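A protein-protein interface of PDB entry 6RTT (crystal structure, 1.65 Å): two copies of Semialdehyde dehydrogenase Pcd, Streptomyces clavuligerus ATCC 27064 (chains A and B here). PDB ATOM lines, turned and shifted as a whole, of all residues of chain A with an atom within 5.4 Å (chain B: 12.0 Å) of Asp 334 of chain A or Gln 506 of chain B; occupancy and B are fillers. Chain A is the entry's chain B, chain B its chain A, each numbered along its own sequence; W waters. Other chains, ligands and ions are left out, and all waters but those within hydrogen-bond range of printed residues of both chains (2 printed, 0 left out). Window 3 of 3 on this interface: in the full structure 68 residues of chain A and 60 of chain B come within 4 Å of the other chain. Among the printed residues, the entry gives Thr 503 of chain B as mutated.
Water W1 lies within hydrogen-bond range of the backbone carbonyl oxygen of Gln 333 of chain A (2.7 Å), the backbone carbonyl oxygen of Thr 336 of chain A (2.8 Å) and the side-chain amide nitrogen of Gln 506 of chain B (3.2 Å). Water W2 lies within hydrogen-bond range of NE2 of Gln 506 of chain B (3.0 Å), N of Ser 110 of chain A (3.0 Å) and OD1 of Asp 334 of chain A (3.4 Å).
Among the printed residues, pairs that only touch across the chains: Ile 108 of chain A with Gln 506 of chain B (3.4 Å), Leu 337 of chain A with Ala 505 of chain B (3.6 Å), Leu 337 of chain A with Phe 510 of chain B (3.9 Å) and Leu 337 of chain A with Gln 506 of chain B (3.96 Å).
Of chain B, only Gln 506 comes within 4 Å of Ile 108 of chain A. Of chain B, only Gln 506 (2.7 Å) comes within 4 Å of Ser 110 of chain A. No residue of chain B comes within 4 Å of Gln 333 of chain A. Of chain B, only Gln 506 (3.4 Å) comes within 4 Å of Thr 336 of chain A. Leu 337 of chain A touches three residues of chain B. Of the printed residues of chain A, Ala 505 of chain B touches Leu 337 (3.6 Å). Of chain A, only Ile 108, Ser 110, Asp 334, Thr 336 and Leu 337 come within 4 Å of Gln 506 of chain B. Printed residues of chain A within 4 Å of Phe 510 of chain B: Leu 337. The nearest residue of chain A that does not touch Gln 506 of chain B is Thr 335 of chain A (5.2 Å). The nearest printed residue of chain A that does not touch Phe 510 of chain B is Thr 335 of chain A (8.1 Å).
Of the 10 printed residues of chain B, 3 touch a printed residue of chain A. Printed residues of chain B that touch a printed residue of chain A: Ala 505, Gln 506 and Phe 510. Hydrophobic or aromatic side chains of chain B within 4 Å of the printed part of chain A: Ala 505 and Phe 510. Printed residues of chain A that touch a printed residue of chain B: Ile 108, Ser 110, Asp 334, Thr 336 and Leu 337. Hydrophobic or aromatic side chains of chain A within 4 Å of the printed part of chain B: Ile 108 and Leu 337. Along chain A the printed residues that touch a printed residue of chain B span positions 108 to 337. Among the printed residues, no Asp or Glu carboxylate lies within 4 Å of a Lys or Arg side-chain nitrogen of the other chain.
The side-chain amide oxygen of Gln 506 of chain B is in hydrogen-bond range of the side-chain hydroxyl of Ser 110 of chain A, 2.7 Å away. The backbone carbonyl oxygen (O) of Thr 336 of chain A is in hydrogen-bond range of the side-chain amide nitrogen (NE2) of Gln 506 of chain B, 3.4 Å away. O of Asp 334 of chain A sits at hydrogen-bond distance from NE2 of Gln 506 of chain B.
No position is printed for both chains.
The side-chain hydroxyl (OG1) of Thr 336 of chain A sits close to the backbone carbonyl oxygen (O) of Gln 333 of chain A (3.5 Å).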
ATOM      1  N   ILE A 108       8.004 -32.696   3.627  1.00  0.00           N
ATOM      2  CA  ILE A 108       8.457 -33.104   4.957  1.00  0.00           C
ATOM      3  C   ILE A 108       7.405 -32.736   6.001  1.00  0.00           C
ATOM      4  O   ILE A 108       6.571 -31.843   5.808  1.00  0.00           O
ATOM      5  CB  ILE A 108       9.824 -32.483   5.292  1.00  0.00           C
ATOM      6  CG1 ILE A 108       9.729 -30.959   5.458  1.00  0.00           C
ATOM      7  CG2 ILE A 108      10.858 -32.824   4.197  1.00  0.00           C
ATOM      8  CD1 ILE A 108      11.071 -30.330   5.779  1.00  0.00           C
ATOM      9  N   ARG A 109       7.447 -33.443   7.134  1.00  0.00           N
ATOM     10  CA  ARG A 109       6.330 -33.347   8.075  1.00  0.00           C
ATOM     11  C   ARG A 109       6.180 -31.939   8.625  1.00  0.00           C
ATOM     12  O   ARG A 109       5.057 -31.478   8.849  1.00  0.00           O
ATOM     13  CB  ARG A 109       6.487 -34.332   9.224  1.00  0.00           C
ATOM     14  CG  ARG A 109       7.893 -34.659   9.543  1.00  0.00           C
ATOM     15  CD  ARG A 109       7.935 -36.079   9.982  1.00  0.00           C
ATOM     16  NE  ARG A 109       7.237 -36.322  11.248  1.00  0.00           N
ATOM     17  CZ  ARG A 109       6.967 -37.527  11.755  1.00  0.00           C
ATOM     18  NH1 ARG A 109       7.285 -38.620  11.094  1.00  0.00           N
ATOM     19  NH2 ARG A 109       6.343 -37.610  12.919  1.00  0.00           N
ATOM     20  N   SER A 110       7.295 -31.240   8.863  1.00  0.00           N
ATOM     21  CA  SER A 110       7.181 -29.888   9.399  1.00  0.00           C
ATOM     22  C   SER A 110       6.442 -28.981   8.426  1.00  0.00           C
ATOM     23  O   SER A 110       5.667 -28.118   8.845  1.00  0.00           O
ATOM     24  CB  SER A 110       8.555 -29.308   9.721  1.00  0.00           C
ATOM     25  OG  SER A 110       9.329 -29.107   8.550  1.00  0.00           O
ATOM     26  N   PHE A 332       9.099 -38.346   6.290  1.00  0.00           N
ATOM     27  CA  PHE A 332       8.667 -38.607   7.659  1.00  0.00           C
ATOM     28  C   PHE A 332       9.821 -38.565   8.663  1.00  0.00           C
ATOM     29  O   PHE A 332       9.570 -38.580   9.875  1.00  0.00           O
ATOM     30  CB  PHE A 332       7.951 -39.962   7.747  1.00  0.00           C
ATOM     31  CG  PHE A 332       6.497 -39.920   7.353  1.00  0.00           C
ATOM     32  CD1 PHE A 332       5.587 -39.156   8.071  1.00  0.00           C
ATOM     33  CD2 PHE A 332       6.036 -40.665   6.283  1.00  0.00           C
ATOM     34  CE1 PHE A 332       4.251 -39.134   7.716  1.00  0.00           C
ATOM     35  CE2 PHE A 332       4.700 -40.649   5.923  1.00  0.00           C
ATOM     36  CZ  PHE A 332       3.804 -39.881   6.645  1.00  0.00           C
ATOM     37  N   GLN A 333      11.067 -38.508   8.206  1.00  0.00           N
ATOM     38  CA  GLN A 333      12.212 -38.377   9.102  1.00  0.00           C
ATOM     39  C   GLN A 333      12.490 -36.904   9.353  1.00  0.00           C
ATOM     40  O   GLN A 333      12.635 -36.125   8.405  1.00  0.00           O
ATOM     41  CB  GLN A 333      13.453 -39.047   8.507  1.00  0.00           C
ATOM     42  CG  GLN A 333      13.308 -40.546   8.281  1.00  0.00           C
ATOM     43  CD  GLN A 333      13.403 -41.338   9.567  1.00  0.00           C
ATOM     44  OE1 GLN A 333      13.624 -40.779  10.643  1.00  0.00           O
ATOM     45  NE2 GLN A 333      13.233 -42.650   9.463  1.00  0.00           N
ATOM     46  N   ASP A 334      12.586 -36.527  10.632  1.00  0.00           N
ATOM     47  CA  ASP A 334      12.795 -35.124  10.965  1.00  0.00           C
ATOM     48  C   ASP A 334      14.122 -34.578  10.456  1.00  0.00           C
ATOM     49  O   ASP A 334      14.250 -33.361  10.291  1.00  0.00           O
ATOM     50  CB  ASP A 334      12.720 -34.919  12.474  1.00  0.00           C
ATOM     51  CG  ASP A 334      11.296 -34.789  12.966  1.00  0.00           C
ATOM     52  OD1 ASP A 334      10.476 -34.148  12.260  1.00  0.00           O
ATOM     53  OD2 ASP A 334      11.008 -35.316  14.056  1.00  0.00           O
ATOM     54  N   THR A 335      15.114 -35.439  10.220  1.00  0.00           N
ATOM     55  CA  THR A 335      16.389 -34.977   9.685  1.00  0.00           C
ATOM     56  C   THR A 335      16.299 -34.561   8.221  1.00  0.00           C
ATOM     57  O   THR A 335      17.202 -33.884   7.729  1.00  0.00           O
ATOM     58  CB  THR A 335      17.447 -36.071   9.820  1.00  0.00           C
ATOM     59  OG1 THR A 335      16.936 -37.295   9.285  1.00  0.00           O
ATOM     60  CG2 THR A 335      17.811 -36.267  11.286  1.00  0.00           C
ATOM     61  N   THR A 336      15.256 -34.967   7.517  1.00  0.00           N
ATOM     62  CA  THR A 336      15.142 -34.656   6.096  1.00  0.00           C
ATOM     63  C   THR A 336      14.795 -33.189   5.883  1.00  0.00           C
ATOM     64  O   THR A 336      13.898 -32.658   6.540  1.00  0.00           O
ATOM     65  CB  THR A 336      14.068 -35.528   5.459  1.00  0.00           C
ATOM     66  OG1 THR A 336      14.458 -36.907   5.553  1.00  0.00           O
ATOM     67  CG2 THR A 336      13.840 -35.140   3.982  1.00  0.00           C
ATOM     68  N   LEU A 337      15.482 -32.551   4.935  1.00  0.00           N
ATOM     69  CA  LEU A 337      15.078 -31.253   4.405  1.00  0.00           C
ATOM     70  C   LEU A 337      14.422 -31.370   3.032  1.00  0.00           C
ATOM     71  O   LEU A 337      13.422 -30.692   2.767  1.00  0.00           O
ATOM     72  CB  LEU A 337      16.287 -30.312   4.323  1.00  0.00           C
ATOM     73  CG  LEU A 337      16.020 -28.914   3.754  1.00  0.00           C
ATOM     74  CD1 LEU A 337      14.961 -28.203   4.589  1.00  0.00           C
ATOM     75  CD2 LEU A 337      17.291 -28.075   3.688  1.00  0.00           C
ATOM     76  N   VAL B 502      16.804 -15.153   9.551  1.00  0.00           N
ATOM     77  CA  VAL B 502      15.791 -15.922   8.841  1.00  0.00           C
ATOM     78  C   VAL B 502      15.523 -17.201   9.621  1.00  0.00           C
ATOM     79  O   VAL B 502      16.399 -17.720  10.319  1.00  0.00           O
ATOM     80  CB  VAL B 502      16.219 -16.235   7.383  1.00  0.00           C
ATOM     81  CG1 VAL B 502      17.544 -17.007   7.353  1.00  0.00           C
ATOM     82  CG2 VAL B 502      15.150 -17.017   6.649  1.00  0.00           C
ATOM     83  N   THR B 503      14.292 -17.692   9.526  1.00  0.00           N
ATOM     84  CA  THR B 503      13.967 -19.000  10.080  1.00  0.00           C
ATOM     85  C   THR B 503      14.832 -20.065   9.419  1.00  0.00           C
ATOM     86  O   THR B 503      14.959 -20.111   8.191  1.00  0.00           O
ATOM     87  CB  THR B 503      12.485 -19.300   9.876  1.00  0.00           C
ATOM     88  OG1 THR B 503      11.714 -18.330  10.599  1.00  0.00           O
ATOM     89  CG2 THR B 503      12.138 -20.697  10.379  1.00  0.00           C
ATOM     90  N   LEU B 504      15.464 -20.901  10.237  1.00  0.00           N
ATOM     91  CA  LEU B 504      16.357 -21.934   9.726  1.00  0.00           C
ATOM     92  C   LEU B 504      15.551 -23.203   9.493  1.00  0.00           C
ATOM     93  O   LEU B 504      14.895 -23.709  10.415  1.00  0.00           O
ATOM     94  CB  LEU B 504      17.508 -22.189  10.696  1.00  0.00           C
ATOM     95  CG  LEU B 504      18.405 -20.984  10.978  1.00  0.00           C
ATOM     96  CD1 LEU B 504      19.486 -21.371  11.982  1.00  0.00           C
ATOM     97  CD2 LEU B 504      19.026 -20.430   9.704  1.00  0.00           C
ATOM     98  N   ALA B 505      15.586 -23.704   8.261  1.00  0.00           N
ATOM     99  CA  ALA B 505      14.803 -24.881   7.913  1.00  0.00           C
ATOM    100  C   ALA B 505      15.342 -26.089   8.664  1.00  0.00           C
ATOM    101  O   ALA B 505      16.535 -26.415   8.562  1.00  0.00           O
ATOM    102  CB  ALA B 505      14.832 -25.123   6.408  1.00  0.00           C
ATOM    103  N   GLN B 506      14.457 -26.737   9.424  1.00  0.00           N
ATOM    104  CA  GLN B 506      14.792 -27.876  10.276  1.00  0.00           C
ATOM    105  C   GLN B 506      15.842 -27.511  11.325  1.00  0.00           C
ATOM    106  O   GLN B 506      16.521 -28.391  11.872  1.00  0.00           O
ATOM    107  CB  GLN B 506      15.245 -29.076   9.430  1.00  0.00           C
ATOM    108  CG  GLN B 506      14.278 -29.430   8.294  1.00  0.00           C
ATOM    109  CD  GLN B 506      12.866 -29.732   8.780  1.00  0.00           C
ATOM    110  OE1 GLN B 506      11.977 -28.877   8.722  1.00  0.00           O
ATOM    111  NE2 GLN B 506      12.653 -30.950   9.261  1.00  0.00           N
ATOM    112  N   GLY B 507      15.976 -26.216  11.619  1.00  0.00           N
ATOM    113  CA  GLY B 507      16.972 -25.725  12.556  1.00  0.00           C
ATOM    114  C   GLY B 507      18.401 -25.705  12.056  1.00  0.00           C
ATOM    115  O   GLY B 507      19.300 -25.367  12.832  1.00  0.00           O
ATOM    116  N   VAL B 508      18.647 -26.039  10.790  1.00  0.00           N
ATOM    117  CA  VAL B 508      20.001 -26.178  10.260  1.00  0.00           C
ATOM    118  C   VAL B 508      20.516 -24.821   9.799  1.00  0.00           C
ATOM    119  O   VAL B 508      19.849 -24.125   9.025  1.00  0.00           O
ATOM    120  CB  VAL B 508      20.034 -27.192   9.103  1.00  0.00           C
ATOM    121  CG1 VAL B 508      21.433 -27.266   8.504  1.00  0.00           C
ATOM    122  CG2 VAL B 508      19.574 -28.564   9.585  1.00  0.00           C
ATOM    123  N   ASP B 509      21.711 -24.444  10.261  1.00  0.00           N
ATOM    124  CA  ASP B 509      22.391 -23.241   9.782  1.00  0.00           C
ATOM    125  C   ASP B 509      23.430 -23.651   8.746  1.00  0.00           C
ATOM    126  O   ASP B 509      24.436 -24.288   9.079  1.00  0.00           O
ATOM    127  CB  ASP B 509      23.031 -22.465  10.931  1.00  0.00           C
ATOM    128  CG  ASP B 509      23.564 -21.098  10.497  1.00  0.00           C
ATOM    129  OD1 ASP B 509      23.867 -20.906   9.298  1.00  0.00           O
ATOM    130  OD2 ASP B 509      23.682 -20.205  11.367  1.00  0.00           O
ATOM    131  N   PHE B 510      23.199 -23.273   7.487  1.00  0.00           N
ATOM    132  CA  PHE B 510      24.088 -23.656   6.398  1.00  0.00           C
ATOM    133  C   PHE B 510      25.263 -22.706   6.227  1.00  0.00           C
ATOM    134  O   PHE B 510      25.884 -22.696   5.158  1.00  0.00           O
ATOM    135  CB  PHE B 510      23.306 -23.765   5.090  1.00  0.00           C
ATOM    136  CG  PHE B 510      22.486 -25.004   4.997  1.00  0.00           C
ATOM    137  CD1 PHE B 510      23.069 -26.204   4.616  1.00  0.00           C
ATOM    138  CD2 PHE B 510      21.141 -24.989   5.312  1.00  0.00           C
ATOM    139  CE1 PHE B 510      22.324 -27.352   4.539  1.00  0.00           C
ATOM    140  CE2 PHE B 510      20.385 -26.142   5.242  1.00  0.00           C
ATOM    141  CZ  PHE B 510      20.979 -27.329   4.850  1.00  0.00           C
ATOM    142  N   SER B 511      25.600 -21.931   7.251  1.00  0.00           N
ATOM    143  CA  SER B 511      26.702 -20.982   7.142  1.00  0.00           C
ATOM    144  C   SER B 511      27.788 -21.224   8.193  1.00  0.00           C
ATOM    145  O   SER B 511      27.868 -22.298   8.794  1.00  0.00           O
ATOM    146  CB  SER B 511      26.171 -19.550   7.257  1.00  0.00           C
ATOM    147  OG  SER B 511      25.712 -19.285   8.572  1.00  0.00           O
HETATM  148  O   HOH W   1      11.640 -33.655   7.774  1.00  0.00           O
HETATM  149  O   HOH W   2      10.012 -32.294   9.464  1.00  0.00           O
